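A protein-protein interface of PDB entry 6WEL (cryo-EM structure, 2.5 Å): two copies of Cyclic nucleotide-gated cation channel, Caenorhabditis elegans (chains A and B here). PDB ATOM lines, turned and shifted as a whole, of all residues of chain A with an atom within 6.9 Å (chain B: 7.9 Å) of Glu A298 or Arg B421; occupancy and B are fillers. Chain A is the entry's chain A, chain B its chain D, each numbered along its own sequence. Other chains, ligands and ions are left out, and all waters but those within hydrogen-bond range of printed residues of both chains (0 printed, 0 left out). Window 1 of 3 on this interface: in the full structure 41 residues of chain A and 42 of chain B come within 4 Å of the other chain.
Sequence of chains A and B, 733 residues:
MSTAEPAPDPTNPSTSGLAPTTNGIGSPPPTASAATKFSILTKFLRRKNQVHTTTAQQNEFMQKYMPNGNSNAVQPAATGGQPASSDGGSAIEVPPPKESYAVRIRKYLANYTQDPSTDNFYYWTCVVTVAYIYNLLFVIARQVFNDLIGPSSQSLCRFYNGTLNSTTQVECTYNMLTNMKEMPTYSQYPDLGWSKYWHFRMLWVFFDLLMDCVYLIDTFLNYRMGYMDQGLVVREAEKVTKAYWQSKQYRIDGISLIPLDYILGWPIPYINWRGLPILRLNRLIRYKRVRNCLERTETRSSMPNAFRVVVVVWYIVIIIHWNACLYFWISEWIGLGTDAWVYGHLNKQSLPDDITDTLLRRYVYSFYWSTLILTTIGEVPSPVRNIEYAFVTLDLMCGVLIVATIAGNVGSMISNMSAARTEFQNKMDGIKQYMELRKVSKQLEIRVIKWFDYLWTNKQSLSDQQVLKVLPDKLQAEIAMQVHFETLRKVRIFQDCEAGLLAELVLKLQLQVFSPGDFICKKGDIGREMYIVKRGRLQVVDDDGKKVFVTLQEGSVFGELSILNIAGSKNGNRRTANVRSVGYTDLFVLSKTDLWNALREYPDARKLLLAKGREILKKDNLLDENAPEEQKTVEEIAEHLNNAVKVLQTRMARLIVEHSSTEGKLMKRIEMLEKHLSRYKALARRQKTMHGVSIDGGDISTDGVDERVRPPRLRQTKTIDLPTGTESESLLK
The guanidinium group (NE) of Arg B421 is in salt-bridge range of the side-chain carboxylate (OE1) of Glu A298 (3.99 Å).
No position is printed for both chains.
Of the 4 pairs that touch across the chains among the printed residues, none has its exchanged pair printed and touching as well.
The side-chain hydroxyl (OG1) of Thr A299 is in hydrogen-bond range of the backbone carbonyl oxygen (O) of Arg A296.
OE1 of Glu A298 lies within salt-bridge range of NE of Arg A308, 3.7 Å away.
The side-chain hydroxyl of Thr B422 lies within hydrogen-bond range of the backbone carbonyl oxygen of Ser B418 (2.8 Å).
OE1 of Gln B425 sits at hydrogen-bond distance from NH1 of Arg B421 (3.2 Å).
Of the printed residues of chain B, Glu A298 touches Arg B421 (3.9 Å).
Of chain A, only Glu A298, Thr A299 and Arg A308 come within 4 Å of Arg B421.
Of the printed residues of chain B, Arg A308 touches Ser B418 and Arg B421.
Printed residues of chain A within 4 Å of Ser B418: Arg A308.
Of the printed residues of chain B, Thr A299 touches Arg B421.
Leu A294 touches none of the printed residues of chain B.
The nearest residue of chain B that does not touch Glu A298 is Gln B425 (6.1 Å).
The nearest residue of chain A that does not touch Arg B421 is Pro A304 (4.2 Å).
Arg B421 touches Thr A299 (NH1 to CA, 3.95 Å).
NH2 of Arg A308 touches CB of Ser B418 (3.4 Å).
Arg A308 touches Arg B421 (NH2 to CG, 3.95 Å).
Of the 17 printed residues of chain B, 2 touch a printed residue of chain A.
Among the printed residues, 4 pairs touch across the chains.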
ATOM      1  N   TYR A 122      27.962  12.883  -6.250  1.00  0.00           N
ATOM      2  CA  TYR A 122      26.552  12.663  -6.544  1.00  0.00           C
ATOM      3  C   TYR A 122      26.209  11.180  -6.513  1.00  0.00           C
ATOM      4  O   TYR A 122      25.194  10.778  -5.930  1.00  0.00           O
ATOM      5  CB  TYR A 122      26.192  13.275  -7.895  1.00  0.00           C
ATOM      6  CG  TYR A 122      24.830  12.866  -8.396  1.00  0.00           C
ATOM      7  CD1 TYR A 122      23.685  13.445  -7.891  1.00  0.00           C
ATOM      8  CD2 TYR A 122      24.694  11.891  -9.366  1.00  0.00           C
ATOM      9  CE1 TYR A 122      22.452  13.066  -8.334  1.00  0.00           C
ATOM     10  CE2 TYR A 122      23.464  11.508  -9.811  1.00  0.00           C
ATOM     11  CZ  TYR A 122      22.349  12.099  -9.294  1.00  0.00           C
ATOM     12  OH  TYR A 122      21.116  11.719  -9.745  1.00  0.00           O
ATOM     13  N   ASN A 292      19.230  16.298  -0.586  1.00  0.00           N
ATOM     14  CA  ASN A 292      20.257  16.787  -1.493  1.00  0.00           C
ATOM     15  C   ASN A 292      20.325  15.942  -2.753  1.00  0.00           C
ATOM     16  O   ASN A 292      20.378  16.475  -3.863  1.00  0.00           O
ATOM     17  CB  ASN A 292      21.601  16.800  -0.769  1.00  0.00           C
ATOM     18  CG  ASN A 292      22.749  17.218  -1.658  1.00  0.00           C
ATOM     19  OD1 ASN A 292      22.642  18.170  -2.426  1.00  0.00           O
ATOM     20  ND2 ASN A 292      23.863  16.508  -1.554  1.00  0.00           N
ATOM     21  N   CYS A 293      20.335  14.618  -2.607  1.00  0.00           N
ATOM     22  CA  CYS A 293      20.376  13.754  -3.781  1.00  0.00           C
ATOM     23  C   CYS A 293      19.181  13.985  -4.691  1.00  0.00           C
ATOM     24  O   CYS A 293      19.322  13.989  -5.915  1.00  0.00           O
ATOM     25  CB  CYS A 293      20.442  12.292  -3.361  1.00  0.00           C
ATOM     26  SG  CYS A 293      20.206  11.129  -4.696  1.00  0.00           S
ATOM     27  N   LEU A 294      17.992  14.185  -4.120  1.00  0.00           N
ATOM     28  CA  LEU A 294      16.814  14.361  -4.964  1.00  0.00           C
ATOM     29  C   LEU A 294      16.796  15.735  -5.627  1.00  0.00           C
ATOM     30  O   LEU A 294      16.405  15.864  -6.791  1.00  0.00           O
ATOM     31  CB  LEU A 294      15.544  14.134  -4.154  1.00  0.00           C
ATOM     32  CG  LEU A 294      15.372  12.737  -3.563  1.00  0.00           C
ATOM     33  CD1 LEU A 294      14.067  12.667  -2.820  1.00  0.00           C
ATOM     34  CD2 LEU A 294      15.443  11.672  -4.630  1.00  0.00           C
ATOM     35  N   GLU A 295      17.223  16.772  -4.902  1.00  0.00           N
ATOM     36  CA  GLU A 295      17.396  18.087  -5.508  1.00  0.00           C
ATOM     37  C   GLU A 295      18.384  18.038  -6.664  1.00  0.00           C
ATOM     38  O   GLU A 295      18.159  18.663  -7.704  1.00  0.00           O
ATOM     39  CB  GLU A 295      17.875  19.089  -4.463  1.00  0.00           C
ATOM     40  CG  GLU A 295      16.828  19.519  -3.460  1.00  0.00           C
ATOM     41  CD  GLU A 295      17.436  20.205  -2.246  1.00  0.00           C
ATOM     42  OE1 GLU A 295      18.633  20.563  -2.297  1.00  0.00           O
ATOM     43  OE2 GLU A 295      16.723  20.379  -1.237  1.00  0.00           O
ATOM     44  N   ARG A 296      19.489  17.317  -6.497  1.00  0.00           N
ATOM     45  CA  ARG A 296      20.474  17.227  -7.567  1.00  0.00           C
ATOM     46  C   ARG A 296      19.975  16.368  -8.714  1.00  0.00           C
ATOM     47  O   ARG A 296      20.357  16.589  -9.863  1.00  0.00           O
ATOM     48  CB  ARG A 296      21.792  16.690  -7.026  1.00  0.00           C
ATOM     49  CG  ARG A 296      22.483  17.664  -6.110  1.00  0.00           C
ATOM     50  CD  ARG A 296      23.612  17.025  -5.330  1.00  0.00           C
ATOM     51  NE  ARG A 296      24.833  16.906  -6.115  1.00  0.00           N
ATOM     52  CZ  ARG A 296      26.048  16.817  -5.589  1.00  0.00           C
ATOM     53  NH1 ARG A 296      26.208  16.848  -4.277  1.00  0.00           N
ATOM     54  NH2 ARG A 296      27.107  16.709  -6.378  1.00  0.00           N
ATOM     55  N   THR A 297      19.144  15.372  -8.434  1.00  0.00           N
ATOM     56  CA  THR A 297      18.611  14.549  -9.509  1.00  0.00           C
ATOM     57  C   THR A 297      17.581  15.308 -10.326  1.00  0.00           C
ATOM     58  O   THR A 297      17.414  15.036 -11.516  1.00  0.00           O
ATOM     59  CB  THR A 297      18.007  13.272  -8.938  1.00  0.00           C
ATOM     60  OG1 THR A 297      18.957  12.650  -8.074  1.00  0.00           O
ATOM     61  CG2 THR A 297      17.656  12.312 -10.038  1.00  0.00           C
ATOM     62  N   GLU A 298      16.881  16.257  -9.711  1.00  0.00           N
ATOM     63  CA  GLU A 298      15.923  17.050 -10.469  1.00  0.00           C
ATOM     64  C   GLU A 298      16.618  17.981 -11.452  1.00  0.00           C
ATOM     65  O   GLU A 298      16.130  18.181 -12.568  1.00  0.00           O
ATOM     66  CB  GLU A 298      15.028  17.846  -9.530  1.00  0.00           C
ATOM     67  CG  GLU A 298      14.099  18.781 -10.264  1.00  0.00           C
ATOM     68  CD  GLU A 298      12.834  19.081  -9.506  1.00  0.00           C
ATOM     69  OE1 GLU A 298      12.056  19.931  -9.975  1.00  0.00           O
ATOM     70  OE2 GLU A 298      12.609  18.467  -8.448  1.00  0.00           O
ATOM     71  N   THR A 299      17.753  18.565 -11.058  1.00  0.00           N
ATOM     72  CA  THR A 299      18.452  19.492 -11.946  1.00  0.00           C
ATOM     73  C   THR A 299      19.131  18.757 -13.093  1.00  0.00           C
ATOM     74  O   THR A 299      19.132  19.243 -14.228  1.00  0.00           O
ATOM     75  CB  THR A 299      19.479  20.308 -11.172  1.00  0.00           C
ATOM     76  OG1 THR A 299      20.596  19.476 -10.847  1.00  0.00           O
ATOM     77  CG2 THR A 299      18.879  20.851  -9.903  1.00  0.00           C
ATOM     78  N   ARG A 300      19.716  17.597 -12.821  1.00  0.00           N
ATOM     79  CA  ARG A 300      20.302  16.787 -13.876  1.00  0.00           C
ATOM     80  C   ARG A 300      19.264  16.133 -14.772  1.00  0.00           C
ATOM     81  O   ARG A 300      19.643  15.428 -15.709  1.00  0.00           O
ATOM     82  CB  ARG A 300      21.166  15.683 -13.291  1.00  0.00           C
ATOM     83  CG  ARG A 300      22.257  16.123 -12.385  1.00  0.00           C
ATOM     84  CD  ARG A 300      23.118  14.933 -12.092  1.00  0.00           C
ATOM     85  NE  ARG A 300      24.430  15.316 -11.608  1.00  0.00           N
ATOM     86  CZ  ARG A 300      25.534  14.639 -11.876  1.00  0.00           C
ATOM     87  NH1 ARG A 300      25.481  13.556 -12.636  1.00  0.00           N
ATOM     88  NH2 ARG A 300      26.689  15.051 -11.391  1.00  0.00           N
ATOM     89  N   SER A 301      17.982  16.311 -14.494  1.00  0.00           N
ATOM     90  CA  SER A 301      16.954  15.569 -15.199  1.00  0.00           C
ATOM     91  C   SER A 301      16.561  16.269 -16.489  1.00  0.00           C
ATOM     92  O   SER A 301      16.484  17.501 -16.551  1.00  0.00           O
ATOM     93  CB  SER A 301      15.727  15.394 -14.309  1.00  0.00           C
ATOM     94  OG  SER A 301      14.953  14.296 -14.738  1.00  0.00           O
ATOM     95  N   SER A 302      16.311  15.476 -17.523  1.00  0.00           N
ATOM     96  CA  SER A 302      15.740  15.972 -18.762  1.00  0.00           C
ATOM     97  C   SER A 302      14.225  16.079 -18.698  1.00  0.00           C
ATOM     98  O   SER A 302      13.613  16.574 -19.645  1.00  0.00           O
ATOM     99  CB  SER A 302      16.141  15.064 -19.919  1.00  0.00           C
ATOM    100  OG  SER A 302      15.864  13.715 -19.609  1.00  0.00           O
ATOM    101  N   MET A 303      13.614  15.633 -17.602  1.00  0.00           N
ATOM    102  CA  MET A 303      12.166  15.698 -17.412  1.00  0.00           C
ATOM    103  C   MET A 303      11.876  16.157 -15.992  1.00  0.00           C
ATOM    104  O   MET A 303      11.396  15.389 -15.160  1.00  0.00           O
ATOM    105  CB  MET A 303      11.531  14.340 -17.695  1.00  0.00           C
ATOM    106  CG  MET A 303      11.174  14.115 -19.150  1.00  0.00           C
ATOM    107  SD  MET A 303      10.756  12.408 -19.523  1.00  0.00           S
ATOM    108  CE  MET A 303      12.375  11.654 -19.465  1.00  0.00           C
ATOM    109  N   PRO A 304      12.150  17.422 -15.685  1.00  0.00           N
ATOM    110  CA  PRO A 304      12.089  17.865 -14.287  1.00  0.00           C
ATOM    111  C   PRO A 304      10.683  17.958 -13.705  1.00  0.00           C
ATOM    112  O   PRO A 304      10.530  17.868 -12.485  1.00  0.00           O
ATOM    113  CB  PRO A 304      12.773  19.235 -14.340  1.00  0.00           C
ATOM    114  CG  PRO A 304      12.522  19.703 -15.713  1.00  0.00           C
ATOM    115  CD  PRO A 304      12.584  18.501 -16.582  1.00  0.00           C
ATOM    116  N   ASN A 305       9.657  18.174 -14.527  1.00  0.00           N
ATOM    117  CA  ASN A 305       8.284  18.130 -14.029  1.00  0.00           C
ATOM    118  C   ASN A 305       7.859  16.701 -13.721  1.00  0.00           C
ATOM    119  O   ASN A 305       7.295  16.417 -12.652  1.00  0.00           O
ATOM    120  CB  ASN A 305       7.343  18.744 -15.062  1.00  0.00           C
ATOM    121  CG  ASN A 305       7.242  20.249 -14.954  1.00  0.00           C
ATOM    122  OD1 ASN A 305       7.018  20.794 -13.878  1.00  0.00           O
ATOM    123  ND2 ASN A 305       7.390  20.927 -16.081  1.00  0.00           N
ATOM    124  N   PHE A 307       9.790  14.174 -13.064  1.00  0.00           N
ATOM    125  CA  PHE A 307      10.547  13.660 -11.929  1.00  0.00           C
ATOM    126  C   PHE A 307       9.963  14.150 -10.613  1.00  0.00           C
ATOM    127  O   PHE A 307       9.921  13.408  -9.631  1.00  0.00           O
ATOM    128  CB  PHE A 307      12.020  14.062 -12.053  1.00  0.00           C
ATOM    129  CG  PHE A 307      12.861  13.634 -10.889  1.00  0.00           C
ATOM    130  CD1 PHE A 307      13.317  12.339 -10.791  1.00  0.00           C
ATOM    131  CD2 PHE A 307      13.175  14.523  -9.881  1.00  0.00           C
ATOM    132  CE1 PHE A 307      14.064  11.941  -9.718  1.00  0.00           C
ATOM    133  CE2 PHE A 307      13.918  14.123  -8.808  1.00  0.00           C
ATOM    134  CZ  PHE A 307      14.367  12.834  -8.728  1.00  0.00           C
ATOM    135  N   ARG A 308       9.511  15.398 -10.573  1.00  0.00           N
ATOM    136  CA  ARG A 308       8.905  15.931  -9.363  1.00  0.00           C
ATOM    137  C   ARG A 308       7.628  15.176  -9.006  1.00  0.00           C
ATOM    138  O   ARG A 308       7.411  14.803  -7.844  1.00  0.00           O
ATOM    139  CB  ARG A 308       8.638  17.420  -9.564  1.00  0.00           C
ATOM    140  CG  ARG A 308       7.932  18.112  -8.437  1.00  0.00           C
ATOM    141  CD  ARG A 308       8.385  19.555  -8.324  1.00  0.00           C
ATOM    142  NE  ARG A 308       8.344  20.264  -9.600  1.00  0.00           N
ATOM    143  CZ  ARG A 308       8.694  21.538  -9.757  1.00  0.00           C
ATOM    144  NH1 ARG A 308       8.627  22.108 -10.950  1.00  0.00           N
ATOM    145  NH2 ARG A 308       9.116  22.244  -8.718  1.00  0.00           N
ATOM    146  N   VAL A 311       8.604  11.728  -7.651  1.00  0.00           N
ATOM    147  CA  VAL A 311       9.108  11.736  -6.285  1.00  0.00           C
ATOM    148  C   VAL A 311       7.961  11.893  -5.299  1.00  0.00           C
ATOM    149  O   VAL A 311       7.958  11.273  -4.231  1.00  0.00           O
ATOM    150  CB  VAL A 311      10.174  12.832  -6.124  1.00  0.00           C
ATOM    151  CG1 VAL A 311      10.498  13.066  -4.672  1.00  0.00           C
ATOM    152  CG2 VAL A 311      11.409  12.428  -6.845  1.00  0.00           C
ATOM    153  N   ASN B 416       2.376  27.899  -5.893  1.00  0.00           N
ATOM    154  CA  ASN B 416       3.134  29.061  -5.441  1.00  0.00           C
ATOM    155  C   ASN B 416       4.533  28.679  -4.998  1.00  0.00           C
ATOM    156  O   ASN B 416       5.469  29.461  -5.158  1.00  0.00           O
ATOM    157  CB  ASN B 416       2.417  29.769  -4.297  1.00  0.00           C
ATOM    158  CG  ASN B 416       1.236  30.561  -4.754  1.00  0.00           C
ATOM    159  OD1 ASN B 416       0.351  30.865  -3.971  1.00  0.00           O
ATOM    160  ND2 ASN B 416       1.205  30.896  -6.027  1.00  0.00           N
ATOM    161  N   MET B 417       4.696  27.505  -4.412  1.00  0.00           N
ATOM    162  CA  MET B 417       5.987  27.126  -3.860  1.00  0.00           C
ATOM    163  C   MET B 417       6.913  26.501  -4.886  1.00  0.00           C
ATOM    164  O   MET B 417       8.038  26.142  -4.537  1.00  0.00           O
ATOM    165  CB  MET B 417       5.799  26.177  -2.678  1.00  0.00           C
ATOM    166  CG  MET B 417       5.311  24.806  -3.041  1.00  0.00           C
ATOM    167  SD  MET B 417       5.229  23.711  -1.615  1.00  0.00           S
ATOM    168  CE  MET B 417       4.972  24.906  -0.324  1.00  0.00           C
ATOM    169  N   SER B 418       6.488  26.380  -6.137  1.00  0.00           N
ATOM    170  CA  SER B 418       7.349  25.891  -7.203  1.00  0.00           C
ATOM    171  C   SER B 418       7.429  26.879  -8.357  1.00  0.00           C
ATOM    172  O   SER B 418       7.842  26.508  -9.453  1.00  0.00           O
ATOM    173  CB  SER B 418       6.872  24.531  -7.704  1.00  0.00           C
ATOM    174  OG  SER B 418       5.554  24.594  -8.197  1.00  0.00           O
ATOM    175  N   ALA B 419       7.057  28.136  -8.124  1.00  0.00           N
ATOM    176  CA  ALA B 419       7.023  29.124  -9.191  1.00  0.00           C
ATOM    177  C   ALA B 419       8.419  29.584  -9.586  1.00  0.00           C
ATOM    178  O   ALA B 419       8.678  29.844 -10.766  1.00  0.00           O
ATOM    179  CB  ALA B 419       6.172  30.314  -8.761  1.00  0.00           C
ATOM    180  N   ALA B 420       9.329  29.683  -8.618  1.00  0.00           N
ATOM    181  CA  ALA B 420      10.677  30.159  -8.902  1.00  0.00           C
ATOM    182  C   ALA B 420      11.483  29.128  -9.676  1.00  0.00           C
ATOM    183  O   ALA B 420      12.205  29.473 -10.615  1.00  0.00           O
ATOM    184  CB  ALA B 420      11.378  30.520  -7.601  1.00  0.00           C
ATOM    185  N   ARG B 421      11.384  27.861  -9.288  1.00  0.00           N
ATOM    186  CA  ARG B 421      12.040  26.799 -10.036  1.00  0.00           C
ATOM    187  C   ARG B 421      11.492  26.711 -11.451  1.00  0.00           C
ATOM    188  O   ARG B 421      12.237  26.451 -12.400  1.00  0.00           O
ATOM    189  CB  ARG B 421      11.862  25.480  -9.294  1.00  0.00           C
ATOM    190  CG  ARG B 421      12.247  24.250 -10.064  1.00  0.00           C
ATOM    191  CD  ARG B 421      13.738  24.175 -10.291  1.00  0.00           C
ATOM    192  NE  ARG B 421      14.064  23.135 -11.260  1.00  0.00           N
ATOM    193  CZ  ARG B 421      15.269  22.951 -11.778  1.00  0.00           C
ATOM    194  NH1 ARG B 421      15.465  21.981 -12.660  1.00  0.00           N
ATOM    195  NH2 ARG B 421      16.274  23.736 -11.419  1.00  0.00           N
ATOM    196  N   THR B 422      10.198  26.958 -11.618  1.00  0.00           N
ATOM    197  CA  THR B 422       9.598  26.942 -12.944  1.00  0.00           C
ATOM    198  C   THR B 422      10.116  28.086 -13.800  1.00  0.00           C
ATOM    199  O   THR B 422      10.416  27.897 -14.983  1.00  0.00           O
ATOM    200  CB  THR B 422       8.079  27.007 -12.821  1.00  0.00           C
ATOM    201  OG1 THR B 422       7.616  25.837 -12.148  1.00  0.00           O
ATOM    202  CG2 THR B 422       7.435  27.084 -14.173  1.00  0.00           C
ATOM    203  N   GLU B 423      10.226  29.280 -13.223  1.00  0.00           N
ATOM    204  CA  GLU B 423      10.760  30.416 -13.967  1.00  0.00           C
ATOM    205  C   GLU B 423      12.211  30.183 -14.370  1.00  0.00           C
ATOM    206  O   GLU B 423      12.613  30.480 -15.505  1.00  0.00           O
ATOM    207  CB  GLU B 423      10.626  31.672 -13.121  1.00  0.00           C
ATOM    208  CG  GLU B 423      10.892  32.951 -13.844  1.00  0.00           C
ATOM    209  CD  GLU B 423      10.937  34.122 -12.894  1.00  0.00           C
ATOM    210  OE1 GLU B 423      11.090  33.884 -11.678  1.00  0.00           O
ATOM    211  OE2 GLU B 423      10.819  35.277 -13.352  1.00  0.00           O
ATOM    212  N   PHE B 424      13.010  29.639 -13.455  1.00  0.00           N
ATOM    213  CA  PHE B 424      14.392  29.312 -13.775  1.00  0.00           C
ATOM    214  C   PHE B 424      14.473  28.294 -14.903  1.00  0.00           C
ATOM    215  O   PHE B 424      15.307  28.423 -15.804  1.00  0.00           O
ATOM    216  CB  PHE B 424      15.096  28.787 -12.528  1.00  0.00           C
ATOM    217  CG  PHE B 424      16.470  28.272 -12.789  1.00  0.00           C
ATOM    218  CD1 PHE B 424      17.544  29.133 -12.837  1.00  0.00           C
ATOM    219  CD2 PHE B 424      16.694  26.927 -12.982  1.00  0.00           C
ATOM    220  CE1 PHE B 424      18.803  28.660 -13.081  1.00  0.00           C
ATOM    221  CE2 PHE B 424      17.957  26.456 -13.228  1.00  0.00           C
ATOM    222  CZ  PHE B 424      19.006  27.321 -13.278  1.00  0.00           C
ATOM    223  N   GLN B 425      13.630  27.266 -14.864  1.00  0.00           N
ATOM    224  CA  GLN B 425      13.670  26.251 -15.907  1.00  0.00           C
ATOM    225  C   GLN B 425      13.221  26.816 -17.247  1.00  0.00           C
ATOM    226  O   GLN B 425      13.735  26.420 -18.293  1.00  0.00           O
ATOM    227  CB  GLN B 425      12.813  25.057 -15.502  1.00  0.00           C
ATOM    228  CG  GLN B 425      12.977  23.850 -16.397  1.00  0.00           C
ATOM    229  CD  GLN B 425      14.401  23.334 -16.441  1.00  0.00           C
ATOM    230  OE1 GLN B 425      15.142  23.441 -15.469  1.00  0.00           O
ATOM    231  NE2 GLN B 425      14.791  22.772 -17.575  1.00  0.00           N
ATOM    232  N   ASN B 426      12.278  27.757 -17.235  1.00  0.00           N
ATOM    233  CA  ASN B 426      11.894  28.430 -18.470  1.00  0.00           C
ATOM    234  C   ASN B 426      13.065  29.187 -19.077  1.00  0.00           C
ATOM    235  O   ASN B 426      13.307  29.106 -20.287  1.00  0.00           O
ATOM    236  CB  ASN B 426      10.745  29.397 -18.212  1.00  0.00           C
ATOM    237  CG  ASN B 426       9.462  28.697 -17.911  1.00  0.00           C
ATOM    238  OD1 ASN B 426       9.305  27.518 -18.200  1.00  0.00           O
ATOM    239  ND2 ASN B 426       8.520  29.423 -17.334  1.00  0.00           N
ATOM    240  N   LYS B 427      13.789  29.948 -18.252  1.00  0.00           N
ATOM    241  CA  LYS B 427      14.941  30.686 -18.764  1.00  0.00           C
ATOM    242  C   LYS B 427      16.011  29.748 -19.304  1.00  0.00           C
ATOM    243  O   LYS B 427      16.579  29.990 -20.375  1.00  0.00           O
ATOM    244  CB  LYS B 427      15.519  31.577 -17.674  1.00  0.00           C
ATOM    245  CG  LYS B 427      14.607  32.693 -17.264  1.00  0.00           C
ATOM    246  CD  LYS B 427      15.178  33.454 -16.097  1.00  0.00           C
ATOM    247  CE  LYS B 427      14.165  34.419 -15.539  1.00  0.00           C
ATOM    248  NZ  LYS B 427      13.587  35.258 -16.610  1.00  0.00           N
ATOM    249  N   MET B 428      16.298  28.671 -18.580  1.00  0.00           N
ATOM    250  CA  MET B 428      17.302  27.718 -19.037  1.00  0.00           C
ATOM    251  C   MET B 428      16.889  27.066 -20.350  1.00  0.00           C
ATOM    252  O   MET B 428      17.720  26.873 -21.247  1.00  0.00           O
ATOM    253  CB  MET B 428      17.538  26.667 -17.956  1.00  0.00           C
ATOM    254  CG  MET B 428      18.482  25.569 -18.358  1.00  0.00           C
ATOM    255  SD  MET B 428      20.210  26.035 -18.226  1.00  0.00           S
ATOM    256  CE  MET B 428      20.437  25.926 -16.457  1.00  0.00           C
ATOM    257  N   ASP B 453      23.510  27.087 -13.448  1.00  0.00           N
ATOM    258  CA  ASP B 453      23.243  26.212 -12.313  1.00  0.00           C
ATOM    259  C   ASP B 453      23.866  26.749 -11.032  1.00  0.00           C
ATOM    260  O   ASP B 453      23.263  26.656  -9.962  1.00  0.00           O
ATOM    261  CB  ASP B 453      23.755  24.805 -12.603  1.00  0.00           C
ATOM    262  CG  ASP B 453      22.825  24.014 -13.504  1.00  0.00           C
ATOM    263  OD1 ASP B 453      21.744  24.527 -13.850  1.00  0.00           O
ATOM    264  OD2 ASP B 453      23.172  22.874 -13.868  1.00  0.00           O
ATOM    265  N   TRP B 456      21.737  29.474  -9.740  1.00  0.00           N
ATOM    266  CA  TRP B 456      20.556  28.916  -9.094  1.00  0.00           C
ATOM    267  C   TRP B 456      20.879  28.420  -7.692  1.00  0.00           C
ATOM    268  O   TRP B 456      20.343  28.927  -6.706  1.00  0.00           O
ATOM    269  CB  TRP B 456      19.967  27.793  -9.942  1.00  0.00           C
ATOM    270  CG  TRP B 456      18.795  27.104  -9.325  1.00  0.00           C
ATOM    271  CD1 TRP B 456      18.700  25.785  -9.014  1.00  0.00           C
ATOM    272  CD2 TRP B 456      17.548  27.696  -8.951  1.00  0.00           C
ATOM    273  NE1 TRP B 456      17.475  25.515  -8.466  1.00  0.00           N
ATOM    274  CE2 TRP B 456      16.748  26.674  -8.417  1.00  0.00           C
ATOM    275  CE3 TRP B 456      17.032  28.990  -9.012  1.00  0.00           C
ATOM    276  CZ2 TRP B 456      15.463  26.905  -7.948  1.00  0.00           C
ATOM    277  CZ3 TRP B 456      15.760  29.215  -8.548  1.00  0.00           C
ATOM    278  CH2 TRP B 456      14.991  28.180  -8.021  1.00  0.00           C
ATOM    279  N   THR B 457      21.795  27.464  -7.575  1.00  0.00           N
ATOM    280  CA  THR B 457      22.041  26.846  -6.276  1.00  0.00           C
ATOM    281  C   THR B 457      22.768  27.756  -5.304  1.00  0.00           C
ATOM    282  O   THR B 457      23.279  27.258  -4.299  1.00  0.00           O
ATOM    283  CB  THR B 457      22.840  25.553  -6.425  1.00  0.00           C
ATOM    284  OG1 THR B 457      24.215  25.864  -6.659  1.00  0.00           O
ATOM    285  CG2 THR B 457      22.308  24.723  -7.572  1.00  0.00           C
ATOM    286  N   LYS B 459      21.407  31.282  -5.038  1.00  0.00           N
ATOM    287  CA  LYS B 459      20.408  32.315  -4.764  1.00  0.00           C
ATOM    288  C   LYS B 459      20.974  33.722  -4.962  1.00  0.00           C
ATOM    289  O   LYS B 459      21.122  34.498  -4.018  1.00  0.00           O
ATOM    290  CB  LYS B 459      19.848  32.153  -3.350  1.00  0.00           C
ATOM    291  CG  LYS B 459      19.385  30.752  -3.010  1.00  0.00           C
ATOM    292  CD  LYS B 459      18.000  30.471  -3.570  1.00  0.00           C
ATOM    293  CE  LYS B 459      18.051  29.620  -4.822  1.00  0.00           C
ATOM    294  NZ  LYS B 459      16.700  29.244  -5.293  1.00  0.00           N
